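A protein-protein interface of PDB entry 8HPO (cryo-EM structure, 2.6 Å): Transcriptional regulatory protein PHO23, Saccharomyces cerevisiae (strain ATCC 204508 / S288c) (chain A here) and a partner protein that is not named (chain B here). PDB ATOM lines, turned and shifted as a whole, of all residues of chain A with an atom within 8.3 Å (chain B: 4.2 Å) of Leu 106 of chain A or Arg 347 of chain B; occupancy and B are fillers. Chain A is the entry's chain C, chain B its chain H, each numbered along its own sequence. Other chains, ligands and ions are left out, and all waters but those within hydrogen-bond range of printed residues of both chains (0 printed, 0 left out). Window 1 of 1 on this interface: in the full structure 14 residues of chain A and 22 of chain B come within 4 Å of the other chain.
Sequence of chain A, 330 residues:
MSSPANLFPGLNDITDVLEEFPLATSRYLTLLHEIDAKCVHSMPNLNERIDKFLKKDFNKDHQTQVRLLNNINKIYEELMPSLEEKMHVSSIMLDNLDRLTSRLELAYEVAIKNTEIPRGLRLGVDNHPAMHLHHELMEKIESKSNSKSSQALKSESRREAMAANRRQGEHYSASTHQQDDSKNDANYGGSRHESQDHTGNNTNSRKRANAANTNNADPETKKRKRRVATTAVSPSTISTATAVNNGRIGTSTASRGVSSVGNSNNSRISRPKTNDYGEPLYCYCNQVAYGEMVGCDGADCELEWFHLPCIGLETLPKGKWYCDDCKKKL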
ATOM      1  N   PRO A   9      30.604 -18.516 -22.795  1.00  0.00           N
ATOM      2  CA  PRO A   9      30.450 -19.890 -22.287  1.00  0.00           C
ATOM      3  C   PRO A   9      29.161 -20.554 -22.733  1.00  0.00           C
ATOM      4  O   PRO A   9      29.134 -21.777 -22.939  1.00  0.00           O
ATOM      5  CB  PRO A   9      30.498 -19.701 -20.768  1.00  0.00           C
ATOM      6  CG  PRO A   9      30.027 -18.327 -20.540  1.00  0.00           C
ATOM      7  CD  PRO A   9      30.340 -17.510 -21.754  1.00  0.00           C
ATOM      8  N   GLY A  10      28.088 -19.776 -22.884  1.00  0.00           N
ATOM      9  CA  GLY A  10      26.841 -20.328 -23.380  1.00  0.00           C
ATOM     10  C   GLY A  10      27.002 -21.032 -24.711  1.00  0.00           C
ATOM     11  O   GLY A  10      26.640 -22.199 -24.852  1.00  0.00           O
ATOM     12  N   ASP A  13      29.222 -24.309 -24.512  1.00  0.00           N
ATOM     13  CA  ASP A  13      28.489 -25.458 -23.998  1.00  0.00           C
ATOM     14  C   ASP A  13      27.385 -25.887 -24.952  1.00  0.00           C
ATOM     15  O   ASP A  13      27.089 -27.079 -25.047  1.00  0.00           O
ATOM     16  CB  ASP A  13      27.912 -25.155 -22.617  1.00  0.00           C
ATOM     17  CG  ASP A  13      27.571 -26.419 -21.842  1.00  0.00           C
ATOM     18  OD1 ASP A  13      26.482 -26.477 -21.234  1.00  0.00           O
ATOM     19  OD2 ASP A  13      28.389 -27.361 -21.847  1.00  0.00           O
ATOM     20  N   ILE A  14      26.776 -24.944 -25.674  1.00  0.00           N
ATOM     21  CA  ILE A  14      25.756 -25.302 -26.654  1.00  0.00           C
ATOM     22  C   ILE A  14      26.360 -26.146 -27.764  1.00  0.00           C
ATOM     23  O   ILE A  14      25.757 -27.128 -28.210  1.00  0.00           O
ATOM     24  CB  ILE A  14      25.077 -24.041 -27.216  1.00  0.00           C
ATOM     25  CG1 ILE A  14      24.068 -23.476 -26.225  1.00  0.00           C
ATOM     26  CG2 ILE A  14      24.362 -24.356 -28.501  1.00  0.00           C
ATOM     27  CD1 ILE A  14      23.567 -22.106 -26.596  1.00  0.00           C
ATOM     28  N   VAL A  17      26.864 -29.645 -26.342  1.00  0.00           N
ATOM     29  CA  VAL A  17      25.573 -30.325 -26.244  1.00  0.00           C
ATOM     30  C   VAL A  17      25.128 -30.825 -27.611  1.00  0.00           C
ATOM     31  O   VAL A  17      24.937 -32.028 -27.817  1.00  0.00           O
ATOM     32  CB  VAL A  17      24.510 -29.398 -25.630  1.00  0.00           C
ATOM     33  CG1 VAL A  17      23.176 -30.084 -25.641  1.00  0.00           C
ATOM     34  CG2 VAL A  17      24.867 -29.034 -24.234  1.00  0.00           C
ATOM     35  N   ASP A  98      16.447 -36.359 -21.329  1.00  0.00           N
ATOM     36  CA  ASP A  98      16.033 -35.278 -20.443  1.00  0.00           C
ATOM     37  C   ASP A  98      17.223 -34.639 -19.742  1.00  0.00           C
ATOM     38  O   ASP A  98      17.240 -33.416 -19.539  1.00  0.00           O
ATOM     39  CB  ASP A  98      15.032 -35.788 -19.413  1.00  0.00           C
ATOM     40  CG  ASP A  98      14.493 -34.678 -18.526  1.00  0.00           C
ATOM     41  OD1 ASP A  98      14.433 -33.518 -18.988  1.00  0.00           O
ATOM     42  OD2 ASP A  98      14.133 -34.963 -17.365  1.00  0.00           O
ATOM     43  N   ARG A  99      18.223 -35.441 -19.373  1.00  0.00           N
ATOM     44  CA  ARG A  99      19.476 -34.872 -18.879  1.00  0.00           C
ATOM     45  C   ARG A  99      20.084 -33.923 -19.905  1.00  0.00           C
ATOM     46  O   ARG A  99      20.461 -32.780 -19.588  1.00  0.00           O
ATOM     47  CB  ARG A  99      20.459 -35.994 -18.552  1.00  0.00           C
ATOM     48  CG  ARG A  99      20.554 -36.343 -17.089  1.00  0.00           C
ATOM     49  CD  ARG A  99      21.561 -37.449 -16.887  1.00  0.00           C
ATOM     50  NE  ARG A  99      20.967 -38.764 -17.088  1.00  0.00           N
ATOM     51  CZ  ARG A  99      21.567 -39.755 -17.733  1.00  0.00           C
ATOM     52  NH1 ARG A  99      22.775 -39.572 -18.240  1.00  0.00           N
ATOM     53  NH2 ARG A  99      20.964 -40.925 -17.875  1.00  0.00           N
ATOM     54  N   LEU A 100      20.186 -34.396 -21.152  1.00  0.00           N
ATOM     55  CA  LEU A 100      20.754 -33.568 -22.212  1.00  0.00           C
ATOM     56  C   LEU A 100      19.941 -32.298 -22.423  1.00  0.00           C
ATOM     57  O   LEU A 100      20.503 -31.224 -22.667  1.00  0.00           O
ATOM     58  CB  LEU A 100      20.843 -34.360 -23.509  1.00  0.00           C
ATOM     59  CG  LEU A 100      21.973 -35.375 -23.618  1.00  0.00           C
ATOM     60  CD1 LEU A 100      22.154 -35.802 -25.057  1.00  0.00           C
ATOM     61  CD2 LEU A 100      23.241 -34.793 -23.069  1.00  0.00           C
ATOM     62  N   THR A 101      18.618 -32.393 -22.308  1.00  0.00           N
ATOM     63  CA  THR A 101      17.770 -31.233 -22.531  1.00  0.00           C
ATOM     64  C   THR A 101      17.931 -30.196 -21.431  1.00  0.00           C
ATOM     65  O   THR A 101      17.916 -28.993 -21.703  1.00  0.00           O
ATOM     66  CB  THR A 101      16.319 -31.681 -22.654  1.00  0.00           C
ATOM     67  OG1 THR A 101      16.190 -32.516 -23.807  1.00  0.00           O
ATOM     68  CG2 THR A 101      15.391 -30.496 -22.803  1.00  0.00           C
ATOM     69  N   SER A 102      18.103 -30.628 -20.184  1.00  0.00           N
ATOM     70  CA  SER A 102      18.319 -29.651 -19.120  1.00  0.00           C
ATOM     71  C   SER A 102      19.655 -28.942 -19.292  1.00  0.00           C
ATOM     72  O   SER A 102      19.754 -27.716 -19.114  1.00  0.00           O
ATOM     73  CB  SER A 102      18.250 -30.338 -17.762  1.00  0.00           C
ATOM     74  OG  SER A 102      18.997 -31.537 -17.779  1.00  0.00           O
ATOM     75  N   ARG A 103      20.698 -29.707 -19.639  1.00  0.00           N
ATOM     76  CA  ARG A 103      21.982 -29.123 -20.020  1.00  0.00           C
ATOM     77  C   ARG A 103      21.808 -28.033 -21.073  1.00  0.00           C
ATOM     78  O   ARG A 103      22.224 -26.877 -20.879  1.00  0.00           O
ATOM     79  CB  ARG A 103      22.892 -30.237 -20.541  1.00  0.00           C
ATOM     80  CG  ARG A 103      24.308 -29.851 -20.871  1.00  0.00           C
ATOM     81  CD  ARG A 103      25.249 -30.973 -20.489  1.00  0.00           C
ATOM     82  NE  ARG A 103      26.136 -31.402 -21.568  1.00  0.00           N
ATOM     83  CZ  ARG A 103      27.176 -30.712 -22.020  1.00  0.00           C
ATOM     84  NH1 ARG A 103      27.915 -31.210 -22.994  1.00  0.00           N
ATOM     85  NH2 ARG A 103      27.480 -29.530 -21.511  1.00  0.00           N
ATOM     86  N   LEU A 104      21.195 -28.402 -22.205  1.00  0.00           N
ATOM     87  CA  LEU A 104      20.962 -27.469 -23.303  1.00  0.00           C
ATOM     88  C   LEU A 104      20.238 -26.214 -22.841  1.00  0.00           C
ATOM     89  O   LEU A 104      20.649 -25.104 -23.178  1.00  0.00           O
ATOM     90  CB  LEU A 104      20.160 -28.150 -24.408  1.00  0.00           C
ATOM     91  CG  LEU A 104      20.447 -27.767 -25.860  1.00  0.00           C
ATOM     92  CD1 LEU A 104      19.555 -28.564 -26.778  1.00  0.00           C
ATOM     93  CD2 LEU A 104      20.264 -26.292 -26.114  1.00  0.00           C
ATOM     94  N   GLU A 105      19.126 -26.371 -22.123  1.00  0.00           N
ATOM     95  CA  GLU A 105      18.325 -25.206 -21.766  1.00  0.00           C
ATOM     96  C   GLU A 105      19.072 -24.256 -20.843  1.00  0.00           C
ATOM     97  O   GLU A 105      18.934 -23.034 -20.981  1.00  0.00           O
ATOM     98  CB  GLU A 105      17.007 -25.633 -21.129  1.00  0.00           C
ATOM     99  CG  GLU A 105      16.180 -26.570 -21.980  1.00  0.00           C
ATOM    100  CD  GLU A 105      14.856 -26.922 -21.339  1.00  0.00           C
ATOM    101  OE1 GLU A 105      14.755 -28.010 -20.736  1.00  0.00           O
ATOM    102  OE2 GLU A 105      13.910 -26.115 -21.437  1.00  0.00           O
ATOM    103  N   LEU A 106      19.876 -24.773 -19.908  1.00  0.00           N
ATOM    104  CA  LEU A 106      20.656 -23.853 -19.084  1.00  0.00           C
ATOM    105  C   LEU A 106      21.690 -23.109 -19.919  1.00  0.00           C
ATOM    106  O   LEU A 106      21.868 -21.891 -19.759  1.00  0.00           O
ATOM    107  CB  LEU A 106      21.332 -24.591 -17.931  1.00  0.00           C
ATOM    108  CG  LEU A 106      22.193 -23.685 -17.048  1.00  0.00           C
ATOM    109  CD1 LEU A 106      21.376 -22.572 -16.431  1.00  0.00           C
ATOM    110  CD2 LEU A 106      22.863 -24.497 -15.970  1.00  0.00           C
ATOM    111  N   ALA A 107      22.376 -23.819 -20.823  1.00  0.00           N
ATOM    112  CA  ALA A 107      23.355 -23.156 -21.681  1.00  0.00           C
ATOM    113  C   ALA A 107      22.703 -22.055 -22.512  1.00  0.00           C
ATOM    114  O   ALA A 107      23.220 -20.935 -22.604  1.00  0.00           O
ATOM    115  CB  ALA A 107      24.039 -24.181 -22.581  1.00  0.00           C
ATOM    116  N   TYR A 108      21.563 -22.368 -23.124  1.00  0.00           N
ATOM    117  CA  TYR A 108      20.820 -21.396 -23.917  1.00  0.00           C
ATOM    118  C   TYR A 108      20.422 -20.175 -23.098  1.00  0.00           C
ATOM    119  O   TYR A 108      20.633 -19.032 -23.525  1.00  0.00           O
ATOM    120  CB  TYR A 108      19.581 -22.064 -24.500  1.00  0.00           C
ATOM    121  CG  TYR A 108      18.932 -21.314 -25.631  1.00  0.00           C
ATOM    122  CD1 TYR A 108      19.641 -20.987 -26.772  1.00  0.00           C
ATOM    123  CD2 TYR A 108      17.601 -20.942 -25.561  1.00  0.00           C
ATOM    124  CE1 TYR A 108      19.042 -20.304 -27.808  1.00  0.00           C
ATOM    125  CE2 TYR A 108      16.998 -20.265 -26.589  1.00  0.00           C
ATOM    126  CZ  TYR A 108      17.721 -19.944 -27.708  1.00  0.00           C
ATOM    127  OH  TYR A 108      17.109 -19.263 -28.730  1.00  0.00           O
ATOM    128  N   GLU A 109      19.813 -20.391 -21.935  1.00  0.00           N
ATOM    129  CA  GLU A 109      19.345 -19.249 -21.166  1.00  0.00           C
ATOM    130  C   GLU A 109      20.502 -18.399 -20.673  1.00  0.00           C
ATOM    131  O   GLU A 109      20.340 -17.189 -20.509  1.00  0.00           O
ATOM    132  CB  GLU A 109      18.477 -19.707 -19.997  1.00  0.00           C
ATOM    133  CG  GLU A 109      19.213 -19.907 -18.687  1.00  0.00           C
ATOM    134  CD  GLU A 109      18.281 -20.167 -17.521  1.00  0.00           C
ATOM    135  OE1 GLU A 109      17.854 -19.196 -16.869  1.00  0.00           O
ATOM    136  OE2 GLU A 109      17.967 -21.346 -17.265  1.00  0.00           O
ATOM    137  N   VAL A 110      21.681 -18.987 -20.459  1.00  0.00           N
ATOM    138  CA  VAL A 110      22.792 -18.163 -19.994  1.00  0.00           C
ATOM    139  C   VAL A 110      23.443 -17.440 -21.164  1.00  0.00           C
ATOM    140  O   VAL A 110      23.983 -16.341 -21.003  1.00  0.00           O
ATOM    141  CB  VAL A 110      23.803 -18.997 -19.187  1.00  0.00           C
ATOM    142  CG1 VAL A 110      24.778 -19.727 -20.091  1.00  0.00           C
ATOM    143  CG2 VAL A 110      24.533 -18.106 -18.215  1.00  0.00           C
ATOM    144  N   ALA A 111      23.388 -18.028 -22.362  1.00  0.00           N
ATOM    145  CA  ALA A 111      23.797 -17.294 -23.554  1.00  0.00           C
ATOM    146  C   ALA A 111      22.940 -16.050 -23.747  1.00  0.00           C
ATOM    147  O   ALA A 111      23.457 -14.959 -23.999  1.00  0.00           O
ATOM    148  CB  ALA A 111      23.724 -18.196 -24.781  1.00  0.00           C
ATOM    149  N   ILE A 112      21.620 -16.200 -23.633  1.00  0.00           N
ATOM    150  CA  ILE A 112      20.725 -15.059 -23.821  1.00  0.00           C
ATOM    151  C   ILE A 112      20.845 -14.071 -22.661  1.00  0.00           C
ATOM    152  O   ILE A 112      20.739 -12.855 -22.856  1.00  0.00           O
ATOM    153  CB  ILE A 112      19.278 -15.544 -24.006  1.00  0.00           C
ATOM    154  CG1 ILE A 112      19.141 -16.290 -25.328  1.00  0.00           C
ATOM    155  CG2 ILE A 112      18.312 -14.384 -23.974  1.00  0.00           C
ATOM    156  CD1 ILE A 112      17.935 -17.181 -25.396  1.00  0.00           C
ATOM    157  N   LYS A 113      21.061 -14.571 -21.440  1.00  0.00           N
ATOM    158  CA  LYS A 113      21.182 -13.687 -20.284  1.00  0.00           C
ATOM    159  C   LYS A 113      22.495 -12.920 -20.312  1.00  0.00           C
ATOM    160  O   LYS A 113      22.565 -11.774 -19.855  1.00  0.00           O
ATOM    161  CB  LYS A 113      21.079 -14.488 -18.992  1.00  0.00           C
ATOM    162  CG  LYS A 113      19.679 -14.702 -18.462  1.00  0.00           C
ATOM    163  CD  LYS A 113      19.593 -16.057 -17.785  1.00  0.00           C
ATOM    164  CE  LYS A 113      18.602 -16.045 -16.661  1.00  0.00           C
ATOM    165  NZ  LYS A 113      19.123 -15.281 -15.500  1.00  0.00           N
ATOM    166  N   HIS B 306      27.825 -28.575 -17.217  1.00  0.00           N
ATOM    167  CA  HIS B 306      26.932 -27.442 -17.427  1.00  0.00           C
ATOM    168  C   HIS B 306      27.760 -26.175 -17.254  1.00  0.00           C
ATOM    169  O   HIS B 306      28.989 -26.229 -17.143  1.00  0.00           O
ATOM    170  CB  HIS B 306      25.715 -27.488 -16.500  1.00  0.00           C
ATOM    171  CG  HIS B 306      26.051 -27.589 -15.047  1.00  0.00           C
ATOM    172  ND1 HIS B 306      26.049 -26.498 -14.206  1.00  0.00           N
ATOM    173  CD2 HIS B 306      26.366 -28.656 -14.278  1.00  0.00           C
ATOM    174  CE1 HIS B 306      26.373 -26.884 -12.986  1.00  0.00           C
ATOM    175  NE2 HIS B 306      26.568 -28.190 -13.002  1.00  0.00           N
ATOM    176  N   ILE B 309      27.823 -22.105 -12.036  1.00  0.00           N
ATOM    177  CA  ILE B 309      26.977 -21.077 -11.449  1.00  0.00           C
ATOM    178  C   ILE B 309      27.599 -20.637 -10.126  1.00  0.00           C
ATOM    179  O   ILE B 309      28.474 -21.304  -9.577  1.00  0.00           O
ATOM    180  CB  ILE B 309      25.533 -21.574 -11.256  1.00  0.00           C
ATOM    181  CG1 ILE B 309      25.056 -22.297 -12.508  1.00  0.00           C
ATOM    182  CG2 ILE B 309      24.589 -20.434 -11.000  1.00  0.00           C
ATOM    183  CD1 ILE B 309      24.063 -23.375 -12.223  1.00  0.00           C
ATOM    184  N   CYS B 329      14.566 -19.150  -8.884  1.00  0.00           N
ATOM    185  CA  CYS B 329      13.232 -18.565  -8.854  1.00  0.00           C
ATOM    186  C   CYS B 329      12.160 -19.643  -8.696  1.00  0.00           C
ATOM    187  O   CYS B 329      12.444 -20.842  -8.655  1.00  0.00           O
ATOM    188  CB  CYS B 329      12.972 -17.753 -10.124  1.00  0.00           C
ATOM    189  SG  CYS B 329      12.770 -18.748 -11.617  1.00  0.00           S
ATOM    190  N   GLU B 345      12.668 -22.946 -20.669  1.00  0.00           N
ATOM    191  CA  GLU B 345      12.414 -23.243 -19.256  1.00  0.00           C
ATOM    192  C   GLU B 345      13.376 -22.405 -18.424  1.00  0.00           C
ATOM    193  O   GLU B 345      14.551 -22.753 -18.283  1.00  0.00           O
ATOM    194  CB  GLU B 345      12.532 -24.725 -18.910  1.00  0.00           C
ATOM    195  CG  GLU B 345      11.716 -25.035 -17.654  1.00  0.00           C
ATOM    196  CD  GLU B 345      12.224 -26.207 -16.848  1.00  0.00           C
ATOM    197  OE1 GLU B 345      13.391 -26.606 -17.034  1.00  0.00           O
ATOM    198  OE2 GLU B 345      11.451 -26.716 -16.010  1.00  0.00           O
ATOM    199  N   TYR B 346      12.862 -21.326 -17.849  1.00  0.00           N
ATOM    200  CA  TYR B 346      13.670 -20.234 -17.321  1.00  0.00           C
ATOM    201  C   TYR B 346      13.798 -20.360 -15.805  1.00  0.00           C
ATOM    202  O   TYR B 346      12.790 -20.448 -15.098  1.00  0.00           O
ATOM    203  CB  TYR B 346      13.026 -18.904 -17.709  1.00  0.00           C
ATOM    204  CG  TYR B 346      13.843 -17.655 -17.475  1.00  0.00           C
ATOM    205  CD1 TYR B 346      13.545 -16.799 -16.424  1.00  0.00           C
ATOM    206  CD2 TYR B 346      14.873 -17.302 -18.333  1.00  0.00           C
ATOM    207  CE1 TYR B 346      14.270 -15.643 -16.214  1.00  0.00           C
ATOM    208  CE2 TYR B 346      15.606 -16.149 -18.130  1.00  0.00           C
ATOM    209  CZ  TYR B 346      15.298 -15.321 -17.068  1.00  0.00           C
ATOM    210  OH  TYR B 346      16.016 -14.170 -16.860  1.00  0.00           O
ATOM    211  N   ARG B 347      15.035 -20.379 -15.320  1.00  0.00           N
ATOM    212  CA  ARG B 347      15.405 -20.361 -13.906  1.00  0.00           C
ATOM    213  C   ARG B 347      16.256 -19.124 -13.641  1.00  0.00           C
ATOM    214  O   ARG B 347      16.374 -18.241 -14.491  1.00  0.00           O
ATOM    215  CB  ARG B 347      16.162 -21.632 -13.522  1.00  0.00           C
ATOM    216  CG  ARG B 347      15.777 -22.833 -14.348  1.00  0.00           C
ATOM    217  CD  ARG B 347      16.280 -24.117 -13.729  1.00  0.00           C
ATOM    218  NE  ARG B 347      16.128 -25.250 -14.636  1.00  0.00           N
ATOM    219  CZ  ARG B 347      17.080 -25.682 -15.455  1.00  0.00           C
ATOM    220  NH1 ARG B 347      16.856 -26.714 -16.254  1.00  0.00           N
ATOM    221  NH2 ARG B 347      18.259 -25.080 -15.479  1.00  0.00           N
ATOM    222  N   TYR B 348      16.834 -19.051 -12.441  1.00  0.00           N
ATOM    223  CA  TYR B 348      17.982 -18.181 -12.169  1.00  0.00           C
ATOM    224  C   TYR B 348      17.723 -16.738 -12.613  1.00  0.00           C
ATOM    225  O   TYR B 348      18.255 -16.263 -13.611  1.00  0.00           O
ATOM    226  CB  TYR B 348      19.249 -18.731 -12.831  1.00  0.00           C
ATOM    227  CG  TYR B 348      19.731 -20.018 -12.224  1.00  0.00           C
ATOM    228  CD1 TYR B 348      20.083 -20.084 -10.890  1.00  0.00           C
ATOM    229  CD2 TYR B 348      19.840 -21.165 -12.987  1.00  0.00           C
ATOM    230  CE1 TYR B 348      20.521 -21.253 -10.332  1.00  0.00           C
ATOM    231  CE2 TYR B 348      20.281 -22.342 -12.438  1.00  0.00           C
ATOM    232  CZ  TYR B 348      20.619 -22.383 -11.110  1.00  0.00           C
ATOM    233  OH  TYR B 348      21.059 -23.560 -10.561  1.00  0.00           O
ATOM    234  N   ARG B 349      16.886 -16.061 -11.832  1.00  0.00           N
ATOM    235  CA  ARG B 349      16.340 -14.744 -12.145  1.00  0.00           C
ATOM    236  C   ARG B 349      17.261 -13.833 -12.955  1.00  0.00           C
ATOM    237  O   ARG B 349      16.799 -13.181 -13.895  1.00  0.00           O
ATOM    238  CB  ARG B 349      15.976 -14.018 -10.848  1.00  0.00           C
ATOM    239  CG  ARG B 349      15.314 -14.883  -9.795  1.00  0.00           C
ATOM    240  CD  ARG B 349      13.896 -14.437  -9.523  1.00  0.00           C
ATOM    241  NE  ARG B 349      13.432 -14.910  -8.225  1.00  0.00           N
ATOM    242  CZ  ARG B 349      13.736 -14.329  -7.070  1.00  0.00           C
ATOM    243  NH1 ARG B 349      14.500 -13.246  -7.049  1.00  0.00           N
ATOM    244  NH2 ARG B 349      13.273 -14.828  -5.932  1.00  0.00           N
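The backbone NH of Glu 345 of chain B sits close to the side-chain carboxylate of Glu 105 of chain A (3.5 Å). The backbone NH of Arg 347 of chain B lies within hydrogen-bond range of the side-chain carboxylate of Glu 109 of chain A. The side-chain amino group (NZ) of Lys 113 of chain A lies close to the backbone carbonyl oxygen (O) of Tyr 348 of chain B, 2.3 Å away.
The side-chain carboxylate (OE1) of Glu 345 of chain B is in salt-bridge range of the guanidinium group (NH1) of Arg 347 of chain B (3.6 Å). The side-chain hydroxyl (OH) of Tyr 346 of chain B sits at hydrogen-bond distance from the backbone carbonyl oxygen (O) of Arg 349 of chain B (3.2 Å). OD1 of Asp 13 of chain A is in salt-bridge range of NH2 of Arg 103 of chain A (3.2 Å).
Asp 13 of chain A touches His 306 of chain B (OD1 to CA, 3.95 Å). Leu 106 of chain A touches Arg 347 of chain B. O of Glu 345 of chain B touches OE2 of Glu 109 of chain A (3.8 Å). OE1 of Glu 109 of chain A touches CD2 of Tyr 346 of chain B, at 3.8 Å. Tyr 346 of chain B touches Lys 113 of chain A. Arg 347 of chain B touches Lys 113 of chain A. Lys 113 of chain A touches Arg 349 of chain B (NZ to C, 3.5 Å).
Of the printed residues of chain B, Leu 106 of chain A touches Arg 347 (3.96 Å). Arg 347 of chain B touches three residues of chain A. Of the printed residues of chain A, His 306 of chain B touches Asp 13 (3.95 Å). Printed residues of chain A within 4 Å of Arg 349 of chain B: Lys 113. Thr 101 of chain A touches none of the printed residues of chain B. The nearest residue of chain A that does not touch Arg 347 of chain B is Ser 102 of chain A (4.2 Å).
Of the 21 printed residues of chain A, 5 touch a printed residue of chain B. Hydrophobic or aromatic side chains of chain A that line the printed part of chain B: Leu 106. Among the printed residues, no Asp or Glu carboxylate lies within 4 Å of a Lys or Arg side-chain nitrogen of the other chain.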
